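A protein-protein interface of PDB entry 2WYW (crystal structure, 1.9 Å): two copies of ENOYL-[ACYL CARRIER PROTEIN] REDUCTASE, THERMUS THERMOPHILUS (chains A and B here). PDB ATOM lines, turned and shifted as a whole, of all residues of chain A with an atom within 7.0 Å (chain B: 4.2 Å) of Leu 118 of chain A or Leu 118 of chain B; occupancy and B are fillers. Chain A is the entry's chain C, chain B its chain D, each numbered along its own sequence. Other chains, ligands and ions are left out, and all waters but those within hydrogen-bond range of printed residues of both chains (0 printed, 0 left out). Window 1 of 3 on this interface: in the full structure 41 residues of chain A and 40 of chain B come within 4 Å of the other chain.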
ATOM      1  N   PHE A  96      11.034  12.746   9.348  1.00  0.00           N
ATOM      2  CA  PHE A  96      10.274  12.212  10.450  1.00  0.00           C
ATOM      3  C   PHE A  96      11.254  11.711  11.479  1.00  0.00           C
ATOM      4  O   PHE A  96      12.351  11.199  11.139  1.00  0.00           O
ATOM      5  CB  PHE A  96       9.335  11.075   9.974  1.00  0.00           C
ATOM      6  CG  PHE A  96       8.581  10.388  11.112  1.00  0.00           C
ATOM      7  CD1 PHE A  96       7.531  11.034  11.753  1.00  0.00           C
ATOM      8  CD2 PHE A  96       8.983   9.150  11.586  1.00  0.00           C
ATOM      9  CE1 PHE A  96       6.851  10.424  12.832  1.00  0.00           C
ATOM     10  CE2 PHE A  96       8.298   8.521  12.644  1.00  0.00           C
ATOM     11  CZ  PHE A  96       7.244   9.165  13.273  1.00  0.00           C
ATOM     12  N   ALA A  97      10.855  11.835  12.738  1.00  0.00           N
ATOM     13  CA  ALA A  97      11.505  11.131  13.839  1.00  0.00           C
ATOM     14  C   ALA A  97      10.381  10.785  14.809  1.00  0.00           C
ATOM     15  O   ALA A  97       9.494  11.611  15.000  1.00  0.00           O
ATOM     16  CB  ALA A  97      12.523  12.024  14.512  1.00  0.00           C
ATOM     17  N   TYR A 106      18.551  13.310  23.467  1.00  0.00           N
ATOM     18  CA  TYR A 106      19.206  12.624  22.349  1.00  0.00           C
ATOM     19  C   TYR A 106      19.888  11.313  22.789  1.00  0.00           C
ATOM     20  O   TYR A 106      19.767  10.269  22.127  1.00  0.00           O
ATOM     21  CB  TYR A 106      20.216  13.566  21.648  1.00  0.00           C
ATOM     22  CG  TYR A 106      20.947  12.848  20.550  1.00  0.00           C
ATOM     23  CD1 TYR A 106      20.242  12.330  19.468  1.00  0.00           C
ATOM     24  CD2 TYR A 106      22.317  12.644  20.605  1.00  0.00           C
ATOM     25  CE1 TYR A 106      20.875  11.638  18.463  1.00  0.00           C
ATOM     26  CE2 TYR A 106      22.976  11.928  19.603  1.00  0.00           C
ATOM     27  CZ  TYR A 106      22.239  11.436  18.528  1.00  0.00           C
ATOM     28  OH  TYR A 106      22.828  10.715  17.535  1.00  0.00           O
ATOM     29  N   ASP A 113      14.163   3.848  16.850  1.00  0.00           N
ATOM     30  CA  ASP A 113      13.711   5.218  16.602  1.00  0.00           C
ATOM     31  C   ASP A 113      14.761   6.060  15.847  1.00  0.00           C
ATOM     32  O   ASP A 113      14.429   6.859  14.962  1.00  0.00           O
ATOM     33  CB  ASP A 113      13.344   5.906  17.916  1.00  0.00           C
ATOM     34  CG  ASP A 113      12.046   5.364  18.535  1.00  0.00           C
ATOM     35  OD1 ASP A 113      11.379   4.527  17.879  1.00  0.00           O
ATOM     36  OD2 ASP A 113      11.706   5.774  19.668  1.00  0.00           O
ATOM     37  N   TRP A 114      16.022   5.840  16.199  1.00  0.00           N
ATOM     38  CA  TRP A 114      17.137   6.565  15.615  1.00  0.00           C
ATOM     39  C   TRP A 114      17.336   6.127  14.184  1.00  0.00           C
ATOM     40  O   TRP A 114      17.422   6.956  13.287  1.00  0.00           O
ATOM     41  CB  TRP A 114      18.376   6.276  16.439  1.00  0.00           C
ATOM     42  CG  TRP A 114      19.598   7.072  16.155  1.00  0.00           C
ATOM     43  CD1 TRP A 114      20.066   8.120  16.897  1.00  0.00           C
ATOM     44  CD2 TRP A 114      20.551   6.858  15.110  1.00  0.00           C
ATOM     45  NE1 TRP A 114      21.240   8.586  16.363  1.00  0.00           N
ATOM     46  CE2 TRP A 114      21.570   7.823  15.274  1.00  0.00           C
ATOM     47  CE3 TRP A 114      20.654   5.942  14.059  1.00  0.00           C
ATOM     48  CZ2 TRP A 114      22.676   7.901  14.421  1.00  0.00           C
ATOM     49  CZ3 TRP A 114      21.750   6.018  13.205  1.00  0.00           C
ATOM     50  CH2 TRP A 114      22.748   6.998  13.395  1.00  0.00           C
ATOM     51  N   LEU A 115      17.374   4.821  13.959  1.00  0.00           N
ATOM     52  CA  LEU A 115      17.432   4.293  12.606  1.00  0.00           C
ATOM     53  C   LEU A 115      16.274   4.774  11.703  1.00  0.00           C
ATOM     54  O   LEU A 115      16.506   5.156  10.560  1.00  0.00           O
ATOM     55  CB  LEU A 115      17.490   2.767  12.656  1.00  0.00           C
ATOM     56  CG  LEU A 115      18.815   2.170  13.162  1.00  0.00           C
ATOM     57  CD1 LEU A 115      18.759   0.610  13.215  1.00  0.00           C
ATOM     58  CD2 LEU A 115      19.955   2.611  12.276  1.00  0.00           C
ATOM     59  N   LEU A 116      15.049   4.804  12.223  1.00  0.00           N
ATOM     60  CA  LEU A 116      13.884   5.262  11.428  1.00  0.00           C
ATOM     61  C   LEU A 116      14.007   6.749  11.088  1.00  0.00           C
ATOM     62  O   LEU A 116      13.761   7.169   9.966  1.00  0.00           O
ATOM     63  CB  LEU A 116      12.567   4.985  12.172  1.00  0.00           C
ATOM     64  CG  LEU A 116      11.243   5.293  11.431  1.00  0.00           C
ATOM     65  CD1 LEU A 116      11.104   4.468  10.171  1.00  0.00           C
ATOM     66  CD2 LEU A 116      10.020   5.044  12.372  1.00  0.00           C
ATOM     67  N   ALA A 117      14.429   7.543  12.052  1.00  0.00           N
ATOM     68  CA  ALA A 117      14.689   8.948  11.810  1.00  0.00           C
ATOM     69  C   ALA A 117      15.694   9.156  10.682  1.00  0.00           C
ATOM     70  O   ALA A 117      15.463  10.000   9.830  1.00  0.00           O
ATOM     71  CB  ALA A 117      15.181   9.617  13.091  1.00  0.00           C
ATOM     72  N   LEU A 118      16.808   8.401  10.695  1.00  0.00           N
ATOM     73  CA  LEU A 118      17.854   8.545   9.668  1.00  0.00           C
ATOM     74  C   LEU A 118      17.363   8.021   8.329  1.00  0.00           C
ATOM     75  O   LEU A 118      17.671   8.568   7.280  1.00  0.00           O
ATOM     76  CB  LEU A 118      19.148   7.839  10.073  1.00  0.00           C
ATOM     77  CG  LEU A 118      20.143   8.646  10.936  1.00  0.00           C
ATOM     78  CD1 LEU A 118      20.929   9.646  10.084  1.00  0.00           C
ATOM     79  CD2 LEU A 118      19.480   9.361  12.110  1.00  0.00           C
ATOM     80  N   GLU A 119      16.576   6.965   8.381  1.00  0.00           N
ATOM     81  CA  GLU A 119      16.073   6.329   7.174  1.00  0.00           C
ATOM     82  C   GLU A 119      15.116   7.252   6.425  1.00  0.00           C
ATOM     83  O   GLU A 119      15.239   7.465   5.214  1.00  0.00           O
ATOM     84  CB  GLU A 119      15.357   5.041   7.555  1.00  0.00           C
ATOM     85  CG  GLU A 119      14.954   4.180   6.353  1.00  0.00           C
ATOM     86  CD  GLU A 119      14.178   2.947   6.790  1.00  0.00           C
ATOM     87  OE1 GLU A 119      13.821   2.841   7.995  1.00  0.00           O
ATOM     88  OE2 GLU A 119      13.944   2.098   5.931  1.00  0.00           O
ATOM     89  N   VAL A 120      14.183   7.837   7.164  1.00  0.00           N
ATOM     90  CA  VAL A 120      13.175   8.686   6.558  1.00  0.00           C
ATOM     91  C   VAL A 120      13.721  10.054   6.190  1.00  0.00           C
ATOM     92  O   VAL A 120      13.471  10.551   5.077  1.00  0.00           O
ATOM     93  CB  VAL A 120      11.956   8.847   7.475  1.00  0.00           C
ATOM     94  CG1 VAL A 120      11.013   9.940   6.937  1.00  0.00           C
ATOM     95  CG2 VAL A 120      11.222   7.489   7.583  1.00  0.00           C
ATOM     96  N   SER A 121      14.530  10.629   7.082  1.00  0.00           N
ATOM     97  CA  SER A 121      14.965  12.022   6.913  1.00  0.00           C
ATOM     98  C   SER A 121      16.288  12.202   6.136  1.00  0.00           C
ATOM     99  O   SER A 121      16.532  13.282   5.609  1.00  0.00           O
ATOM    100  CB  SER A 121      15.064  12.708   8.284  1.00  0.00           C
ATOM    101  OG  SER A 121      13.988  12.364   9.110  1.00  0.00           O
ATOM    102  N   ALA A 122      17.108  11.154   6.034  1.00  0.00           N
ATOM    103  CA  ALA A 122      18.396  11.224   5.339  1.00  0.00           C
ATOM    104  C   ALA A 122      18.525  10.201   4.197  1.00  0.00           C
ATOM    105  O   ALA A 122      18.793  10.560   3.033  1.00  0.00           O
ATOM    106  CB  ALA A 122      19.561  11.058   6.369  1.00  0.00           C
ATOM    107  N   TYR A 123      18.323   8.931   4.501  1.00  0.00           N
ATOM    108  CA  TYR A 123      18.485   7.899   3.464  1.00  0.00           C
ATOM    109  C   TYR A 123      17.536   8.125   2.314  1.00  0.00           C
ATOM    110  O   TYR A 123      17.923   7.950   1.174  1.00  0.00           O
ATOM    111  CB  TYR A 123      18.304   6.456   3.987  1.00  0.00           C
ATOM    112  CG  TYR A 123      18.430   5.495   2.846  1.00  0.00           C
ATOM    113  CD1 TYR A 123      19.656   5.286   2.234  1.00  0.00           C
ATOM    114  CD2 TYR A 123      17.302   4.869   2.313  1.00  0.00           C
ATOM    115  CE1 TYR A 123      19.774   4.443   1.118  1.00  0.00           C
ATOM    116  CE2 TYR A 123      17.403   4.039   1.221  1.00  0.00           C
ATOM    117  CZ  TYR A 123      18.636   3.828   0.626  1.00  0.00           C
ATOM    118  OH  TYR A 123      18.707   3.020  -0.460  1.00  0.00           O
ATOM    119  N   SER A 124      16.322   8.603   2.608  1.00  0.00           N
ATOM    120  CA  SER A 124      15.312   8.839   1.576  1.00  0.00           C
ATOM    121  C   SER A 124      15.825   9.660   0.444  1.00  0.00           C
ATOM    122  O   SER A 124      15.398   9.440  -0.682  1.00  0.00           O
ATOM    123  CB  SER A 124      14.056   9.511   2.127  1.00  0.00           C
ATOM    124  OG  SER A 124      14.331  10.735   2.760  1.00  0.00           O
ATOM    125  N   LEU A 125      16.730  10.600   0.730  1.00  0.00           N
ATOM    126  CA  LEU A 125      17.284  11.468  -0.320  1.00  0.00           C
ATOM    127  C   LEU A 125      18.105  10.644  -1.298  1.00  0.00           C
ATOM    128  O   LEU A 125      18.032  10.846  -2.519  1.00  0.00           O
ATOM    129  CB  LEU A 125      18.161  12.585   0.266  1.00  0.00           C
ATOM    130  CG  LEU A 125      18.763  13.538  -0.762  1.00  0.00           C
ATOM    131  CD1 LEU A 125      17.646  14.232  -1.586  1.00  0.00           C
ATOM    132  CD2 LEU A 125      19.650  14.566  -0.098  1.00  0.00           C
ATOM    133  N   VAL A 159      17.537  13.798  17.601  1.00  0.00           N
ATOM    134  CA  VAL A 159      17.976  12.973  16.476  1.00  0.00           C
ATOM    135  C   VAL A 159      17.801  13.657  15.108  1.00  0.00           C
ATOM    136  O   VAL A 159      18.486  13.312  14.143  1.00  0.00           O
ATOM    137  CB  VAL A 159      17.283  11.596  16.463  1.00  0.00           C
ATOM    138  CG1 VAL A 159      15.804  11.726  16.153  1.00  0.00           C
ATOM    139  CG2 VAL A 159      17.983  10.680  15.502  1.00  0.00           C
ATOM    140  N   MET A 160      16.897  14.630  15.018  1.00  0.00           N
ATOM    141  CA  MET A 160      16.669  15.271  13.732  1.00  0.00           C
ATOM    142  C   MET A 160      17.873  16.122  13.357  1.00  0.00           C
ATOM    143  O   MET A 160      18.147  16.289  12.178  1.00  0.00           O
ATOM    144  CB  MET A 160      15.393  16.115  13.709  1.00  0.00           C
ATOM    145  CG  MET A 160      14.978  16.529  12.292  1.00  0.00           C
ATOM    146  SD  MET A 160      14.624  15.170  11.141  1.00  0.00           S
ATOM    147  CE  MET A 160      13.049  14.686  11.855  1.00  0.00           C
ATOM    148  N   ILE A 162      20.938  15.293  13.904  1.00  0.00           N
ATOM    149  CA  ILE A 162      21.883  14.285  13.426  1.00  0.00           C
ATOM    150  C   ILE A 162      21.478  13.813  12.029  1.00  0.00           C
ATOM    151  O   ILE A 162      22.325  13.707  11.126  1.00  0.00           O
ATOM    152  CB  ILE A 162      21.989  13.128  14.432  1.00  0.00           C
ATOM    153  CG1 ILE A 162      22.884  13.527  15.609  1.00  0.00           C
ATOM    154  CG2 ILE A 162      22.639  11.879  13.750  1.00  0.00           C
ATOM    155  CD1 ILE A 162      22.443  14.676  16.422  1.00  0.00           C
ATOM    156  N   ALA A 163      20.171  13.606  11.815  1.00  0.00           N
ATOM    157  CA  ALA A 163      19.648  13.253  10.478  1.00  0.00           C
ATOM    158  C   ALA A 163      19.965  14.354   9.452  1.00  0.00           C
ATOM    159  O   ALA A 163      20.302  14.053   8.329  1.00  0.00           O
ATOM    160  CB  ALA A 163      18.135  12.977  10.538  1.00  0.00           C
ATOM    161  N   LYS A 164      19.868  15.623   9.861  1.00  0.00           N
ATOM    162  CA  LYS A 164      20.168  16.741   8.986  1.00  0.00           C
ATOM    163  C   LYS A 164      21.663  16.884   8.667  1.00  0.00           C
ATOM    164  O   LYS A 164      22.031  17.253   7.552  1.00  0.00           O
ATOM    165  CB  LYS A 164      19.610  18.037   9.580  1.00  0.00           C
ATOM    166  CG  LYS A 164      18.081  18.057   9.705  1.00  0.00           C
ATOM    167  CD  LYS A 164      17.383  17.786   8.351  1.00  0.00           C
ATOM    168  CE  LYS A 164      15.893  18.030   8.412  1.00  0.00           C
ATOM    169  NZ  LYS A 164      15.155  17.844   7.103  1.00  0.00           N
ATOM    170  N   ALA A 165      22.515  16.584   9.627  1.00  0.00           N
ATOM    171  CA  ALA A 165      23.952  16.473   9.353  1.00  0.00           C
ATOM    172  C   ALA A 165      24.196  15.389   8.274  1.00  0.00           C
ATOM    173  O   ALA A 165      24.976  15.595   7.338  1.00  0.00           O
ATOM    174  CB  ALA A 165      24.714  16.130  10.629  1.00  0.00           C
ATOM    175  N   ALA A 166      23.565  14.233   8.443  1.00  0.00           N
ATOM    176  CA  ALA A 166      23.628  13.143   7.441  1.00  0.00           C
ATOM    177  C   ALA A 166      23.086  13.588   6.079  1.00  0.00           C
ATOM    178  O   ALA A 166      23.667  13.283   5.022  1.00  0.00           O
ATOM    179  CB  ALA A 166      22.861  11.894   7.957  1.00  0.00           C
ATOM    180  N   LEU A 167      21.970  14.315   6.106  1.00  0.00           N
ATOM    181  CA  LEU A 167      21.389  14.888   4.900  1.00  0.00           C
ATOM    182  C   LEU A 167      22.312  15.855   4.159  1.00  0.00           C
ATOM    183  O   LEU A 167      22.456  15.763   2.950  1.00  0.00           O
ATOM    184  CB  LEU A 167      20.106  15.630   5.249  1.00  0.00           C
ATOM    185  CG  LEU A 167      19.250  16.132   4.115  1.00  0.00           C
ATOM    186  CD1 LEU A 167      18.595  14.985   3.327  1.00  0.00           C
ATOM    187  CD2 LEU A 167      18.181  17.057   4.705  1.00  0.00           C
ATOM    188  N   TRP B 114      23.278   1.107   4.065  1.00  0.00           N
ATOM    189  CA  TRP B 114      23.331   2.488   4.568  1.00  0.00           C
ATOM    190  C   TRP B 114      22.975   2.501   6.042  1.00  0.00           C
ATOM    191  O   TRP B 114      23.724   3.070   6.870  1.00  0.00           O
ATOM    192  CB  TRP B 114      22.391   3.345   3.770  1.00  0.00           C
ATOM    193  CG  TRP B 114      22.531   4.821   3.948  1.00  0.00           C
ATOM    194  CD1 TRP B 114      23.192   5.691   3.129  1.00  0.00           C
ATOM    195  CD2 TRP B 114      21.908   5.610   4.957  1.00  0.00           C
ATOM    196  NE1 TRP B 114      23.021   6.990   3.581  1.00  0.00           N
ATOM    197  CE2 TRP B 114      22.244   6.960   4.708  1.00  0.00           C
ATOM    198  CE3 TRP B 114      21.076   5.309   6.043  1.00  0.00           C
ATOM    199  CZ2 TRP B 114      21.784   8.003   5.513  1.00  0.00           C
ATOM    200  CZ3 TRP B 114      20.631   6.321   6.841  1.00  0.00           C
ATOM    201  CH2 TRP B 114      20.981   7.676   6.570  1.00  0.00           C
ATOM    202  N   LEU B 115      21.872   1.816   6.381  1.00  0.00           N
ATOM    203  CA  LEU B 115      21.431   1.751   7.761  1.00  0.00           C
ATOM    204  C   LEU B 115      22.482   1.121   8.663  1.00  0.00           C
ATOM    205  O   LEU B 115      22.722   1.630   9.751  1.00  0.00           O
ATOM    206  CB  LEU B 115      20.037   1.084   7.908  1.00  0.00           C
ATOM    207  CG  LEU B 115      18.861   1.955   7.411  1.00  0.00           C
ATOM    208  CD1 LEU B 115      17.558   1.156   7.116  1.00  0.00           C
ATOM    209  CD2 LEU B 115      18.568   3.130   8.375  1.00  0.00           C
ATOM    210  N   LEU B 116      23.133   0.052   8.223  1.00  0.00           N
ATOM    211  CA  LEU B 116      24.091  -0.646   9.088  1.00  0.00           C
ATOM    212  C   LEU B 116      25.329   0.206   9.351  1.00  0.00           C
ATOM    213  O   LEU B 116      25.830   0.251  10.458  1.00  0.00           O
ATOM    214  CB  LEU B 116      24.491  -1.995   8.475  1.00  0.00           C
ATOM    215  CG  LEU B 116      25.503  -2.883   9.238  1.00  0.00           C
ATOM    216  CD1 LEU B 116      25.024  -3.368  10.637  1.00  0.00           C
ATOM    217  CD2 LEU B 116      25.794  -4.075   8.361  1.00  0.00           C
ATOM    218  N   ALA B 117      25.823   0.856   8.310  1.00  0.00           N
ATOM    219  CA  ALA B 117      26.915   1.814   8.412  1.00  0.00           C
ATOM    220  C   ALA B 117      26.621   2.905   9.449  1.00  0.00           C
ATOM    221  O   ALA B 117      27.460   3.191  10.295  1.00  0.00           O
ATOM    222  CB  ALA B 117      27.174   2.449   7.009  1.00  0.00           C
ATOM    223  N   LEU B 118      25.425   3.500   9.381  1.00  0.00           N
ATOM    224  CA  LEU B 118      25.011   4.531  10.336  1.00  0.00           C
ATOM    225  C   LEU B 118      24.827   3.948  11.738  1.00  0.00           C
ATOM    226  O   LEU B 118      25.179   4.594  12.732  1.00  0.00           O
ATOM    227  CB  LEU B 118      23.724   5.240   9.893  1.00  0.00           C
ATOM    228  CG  LEU B 118      23.878   6.446   8.958  1.00  0.00           C
ATOM    229  CD1 LEU B 118      24.386   7.682   9.731  1.00  0.00           C
ATOM    230  CD2 LEU B 118      24.772   6.107   7.757  1.00  0.00           C
ATOM    231  N   GLU B 119      24.313   2.725  11.798  1.00  0.00           N
ATOM    232  CA  GLU B 119      24.047   2.051  13.086  1.00  0.00           C
ATOM    233  C   GLU B 119      25.350   1.754  13.836  1.00  0.00           C
ATOM    234  O   GLU B 119      25.454   2.055  15.022  1.00  0.00           O
ATOM    235  CB  GLU B 119      23.293   0.746  12.847  1.00  0.00           C
ATOM    236  CG  GLU B 119      22.986  -0.082  14.120  1.00  0.00           C
ATOM    237  CD  GLU B 119      22.120  -1.303  13.818  1.00  0.00           C
ATOM    238  OE1 GLU B 119      22.070  -1.724  12.644  1.00  0.00           O
ATOM    239  OE2 GLU B 119      21.489  -1.821  14.752  1.00  0.00           O
ATOM    240  N   VAL B 120      26.325   1.175  13.133  1.00  0.00           N
ATOM    241  CA  VAL B 120      27.617   0.775  13.749  1.00  0.00           C
ATOM    242  C   VAL B 120      28.515   1.995  13.997  1.00  0.00           C
ATOM    243  O   VAL B 120      29.098   2.129  15.067  1.00  0.00           O
ATOM    244  CB  VAL B 120      28.363  -0.314  12.907  1.00  0.00           C
ATOM    245  CG1 VAL B 120      29.749  -0.611  13.455  1.00  0.00           C
ATOM    246  CG2 VAL B 120      27.568  -1.578  12.887  1.00  0.00           C
ATOM    247  N   SER B 121      28.560   2.910  13.030  1.00  0.00           N
ATOM    248  CA  SER B 121      29.521   3.998  13.055  1.00  0.00           C
ATOM    249  C   SER B 121      29.041   5.283  13.761  1.00  0.00           C
ATOM    250  O   SER B 121      29.876   6.089  14.174  1.00  0.00           O
ATOM    251  CB  SER B 121      29.937   4.329  11.627  1.00  0.00           C
ATOM    252  OG  SER B 121      30.320   3.171  10.927  1.00  0.00           O
ATOM    253  N   ALA B 122      27.735   5.500  13.876  1.00  0.00           N
ATOM    254  CA  ALA B 122      27.207   6.706  14.510  1.00  0.00           C
ATOM    255  C   ALA B 122      26.313   6.381  15.707  1.00  0.00           C
ATOM    256  O   ALA B 122      26.577   6.838  16.840  1.00  0.00           O
ATOM    257  CB  ALA B 122      26.469   7.566  13.479  1.00  0.00           C
ATOM    258  N   TYR B 123      25.263   5.586  15.487  1.00  0.00           N
ATOM    259  CA  TYR B 123      24.365   5.221  16.583  1.00  0.00           C
ATOM    260  C   TYR B 123      25.065   4.591  17.767  1.00  0.00           C
ATOM    261  O   TYR B 123      24.696   4.857  18.901  1.00  0.00           O
ATOM    262  CB  TYR B 123      23.224   4.277  16.182  1.00  0.00           C
ATOM    263  CG  TYR B 123      22.355   3.993  17.397  1.00  0.00           C
ATOM    264  CD1 TYR B 123      21.617   5.010  17.983  1.00  0.00           C
ATOM    265  CD2 TYR B 123      22.325   2.750  18.002  1.00  0.00           C
ATOM    266  CE1 TYR B 123      20.855   4.796  19.134  1.00  0.00           C
ATOM    267  CE2 TYR B 123      21.550   2.522  19.151  1.00  0.00           C
ATOM    268  CZ  TYR B 123      20.822   3.552  19.699  1.00  0.00           C
ATOM    269  OH  TYR B 123      20.049   3.363  20.829  1.00  0.00           O
ATOM    270  N   VAL B 159      29.291   6.335   2.197  1.00  0.00           N
ATOM    271  CA  VAL B 159      28.414   6.385   3.382  1.00  0.00           C
ATOM    272  C   VAL B 159      29.195   6.613   4.688  1.00  0.00           C
ATOM    273  O   VAL B 159      28.634   7.158   5.653  1.00  0.00           O
ATOM    274  CB  VAL B 159      27.514   5.136   3.555  1.00  0.00           C
ATOM    275  CG1 VAL B 159      28.325   3.917   3.996  1.00  0.00           C
ATOM    276  CG2 VAL B 159      26.422   5.406   4.567  1.00  0.00           C
ATOM    277  N   ALA B 163      28.100   8.934   7.831  1.00  0.00           N
ATOM    278  CA  ALA B 163      28.104   8.411   9.210  1.00  0.00           C
ATOM    279  C   ALA B 163      28.939   9.305  10.121  1.00  0.00           C
ATOM    280  O   ALA B 163      28.558   9.540  11.253  1.00  0.00           O
ATOM    281  CB  ALA B 163      28.616   6.983   9.258  1.00  0.00           C
ATOM    282  N   ALA B 166      27.051  12.431  11.009  1.00  0.00           N
ATOM    283  CA  ALA B 166      26.114  12.036  12.091  1.00  0.00           C
ATOM    284  C   ALA B 166      26.814  11.891  13.421  1.00  0.00           C
ATOM    285  O   ALA B 166      26.290  12.306  14.441  1.00  0.00           O
ATOM    286  CB  ALA B 166      25.376  10.756  11.754  1.00  0.00           C
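The backbone NH of Tyr 123 of chain B sits at hydrogen-bond distance from the backbone carbonyl oxygen of Leu 118 of chain B, at 2.9 Å.
The indole nitrogen (NE1) of Trp 114 of chain A lies within hydrogen-bond range of the side-chain hydroxyl (OH) of Tyr 106 of chain A (2.9 Å).
The backbone NH (N) of Tyr 123 of chain A lies within hydrogen-bond range of the backbone carbonyl oxygen (O) of Leu 118 of chain A, 2.9 Å away.
O of Glu 119 of chain A is in hydrogen-bond range of N of Ser 124 of chain A (3.0 Å).
Among the printed residues, pairs that only touch across the chains: Trp 114 of chain A with Leu 118 of chain B (3.5 Å), Trp 114 of chain A with Ala 122 of chain B (3.8 Å), Trp 114 of chain A with Tyr 123 of chain B (3.4 Å), Leu 115 of chain A with Leu 115 of chain B (3.6 Å), Leu 115 of chain A with Glu 119 of chain B (3.9 Å), Leu 118 of chain A with Trp 114 of chain B (3.5 Å), Leu 118 of chain A with Leu 118 of chain B (3.99 Å), Glu 119 of chain A with Leu 115 of chain B (3.8 Å), Ala 122 of chain A with Trp 114 of chain B (3.7 Å), Tyr 123 of chain A with Trp 114 of chain B (3.4 Å) and Ile 162 of chain A with Ala 166 of chain B (3.6 Å).
Printed residues of chain A within 4 Å of Leu 118 of chain B: Trp 114 (3.5 Å) and Leu 118 (3.99 Å).
Of the printed residues of chain A, Ala 122 of chain B touches Trp 114.
Printed residues of chain A within 4 Å of Ala 166 of chain B: Ile 162.
The nearest printed residue of chain B that does not touch Leu 118 of chain A is Ala 166 of chain B (4.9 Å).
Of the 24 printed residues of chain A, 7 touch a printed residue of chain B.
Hydrophobic or aromatic side chains of chain A within 4 Å of the printed part of chain B: Trp 114, Leu 115, Leu 118, Ala 122, Tyr 123 and Ile 162.
Of the 13 printed residues of chain B, 7 touch a printed residue of chain A.
Printed residues of chain B that touch a printed residue of chain A: Trp 114, Leu 115, Leu 118, Glu 119, Ala 122, Tyr 123 and Ala 166.
Hydrophobic or aromatic side chains of chain B that line the printed part of chain A: Trp 114, Leu 115, Leu 118, Ala 122, Tyr 123 and Ala 166.
Among the printed residues, no Asp or Glu carboxylate lies within 4 Å of a Lys or Arg side-chain nitrogen of the other chain.
Trp 114 of chain A touches Leu 118 of chain B, and with the chains exchanged Leu 118 of chain A touches Trp 114 of chain B.
Trp 114 of chain A touches Ala 122 of chain B, and with the chains exchanged Ala 122 of chain A touches Trp 114 of chain B.
Trp 114 of chain A touches Tyr 123 of chain B, and with the chains exchanged Tyr 123 of chain A touches Trp 114 of chain B.
Leu 115 of chain B touches its own counterpart, Leu 115 of chain A.
Positions printed for both chains: 114, 115, 116, 117, 118, 119, 120, 121, 122, 123, 159, 163 and 166.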
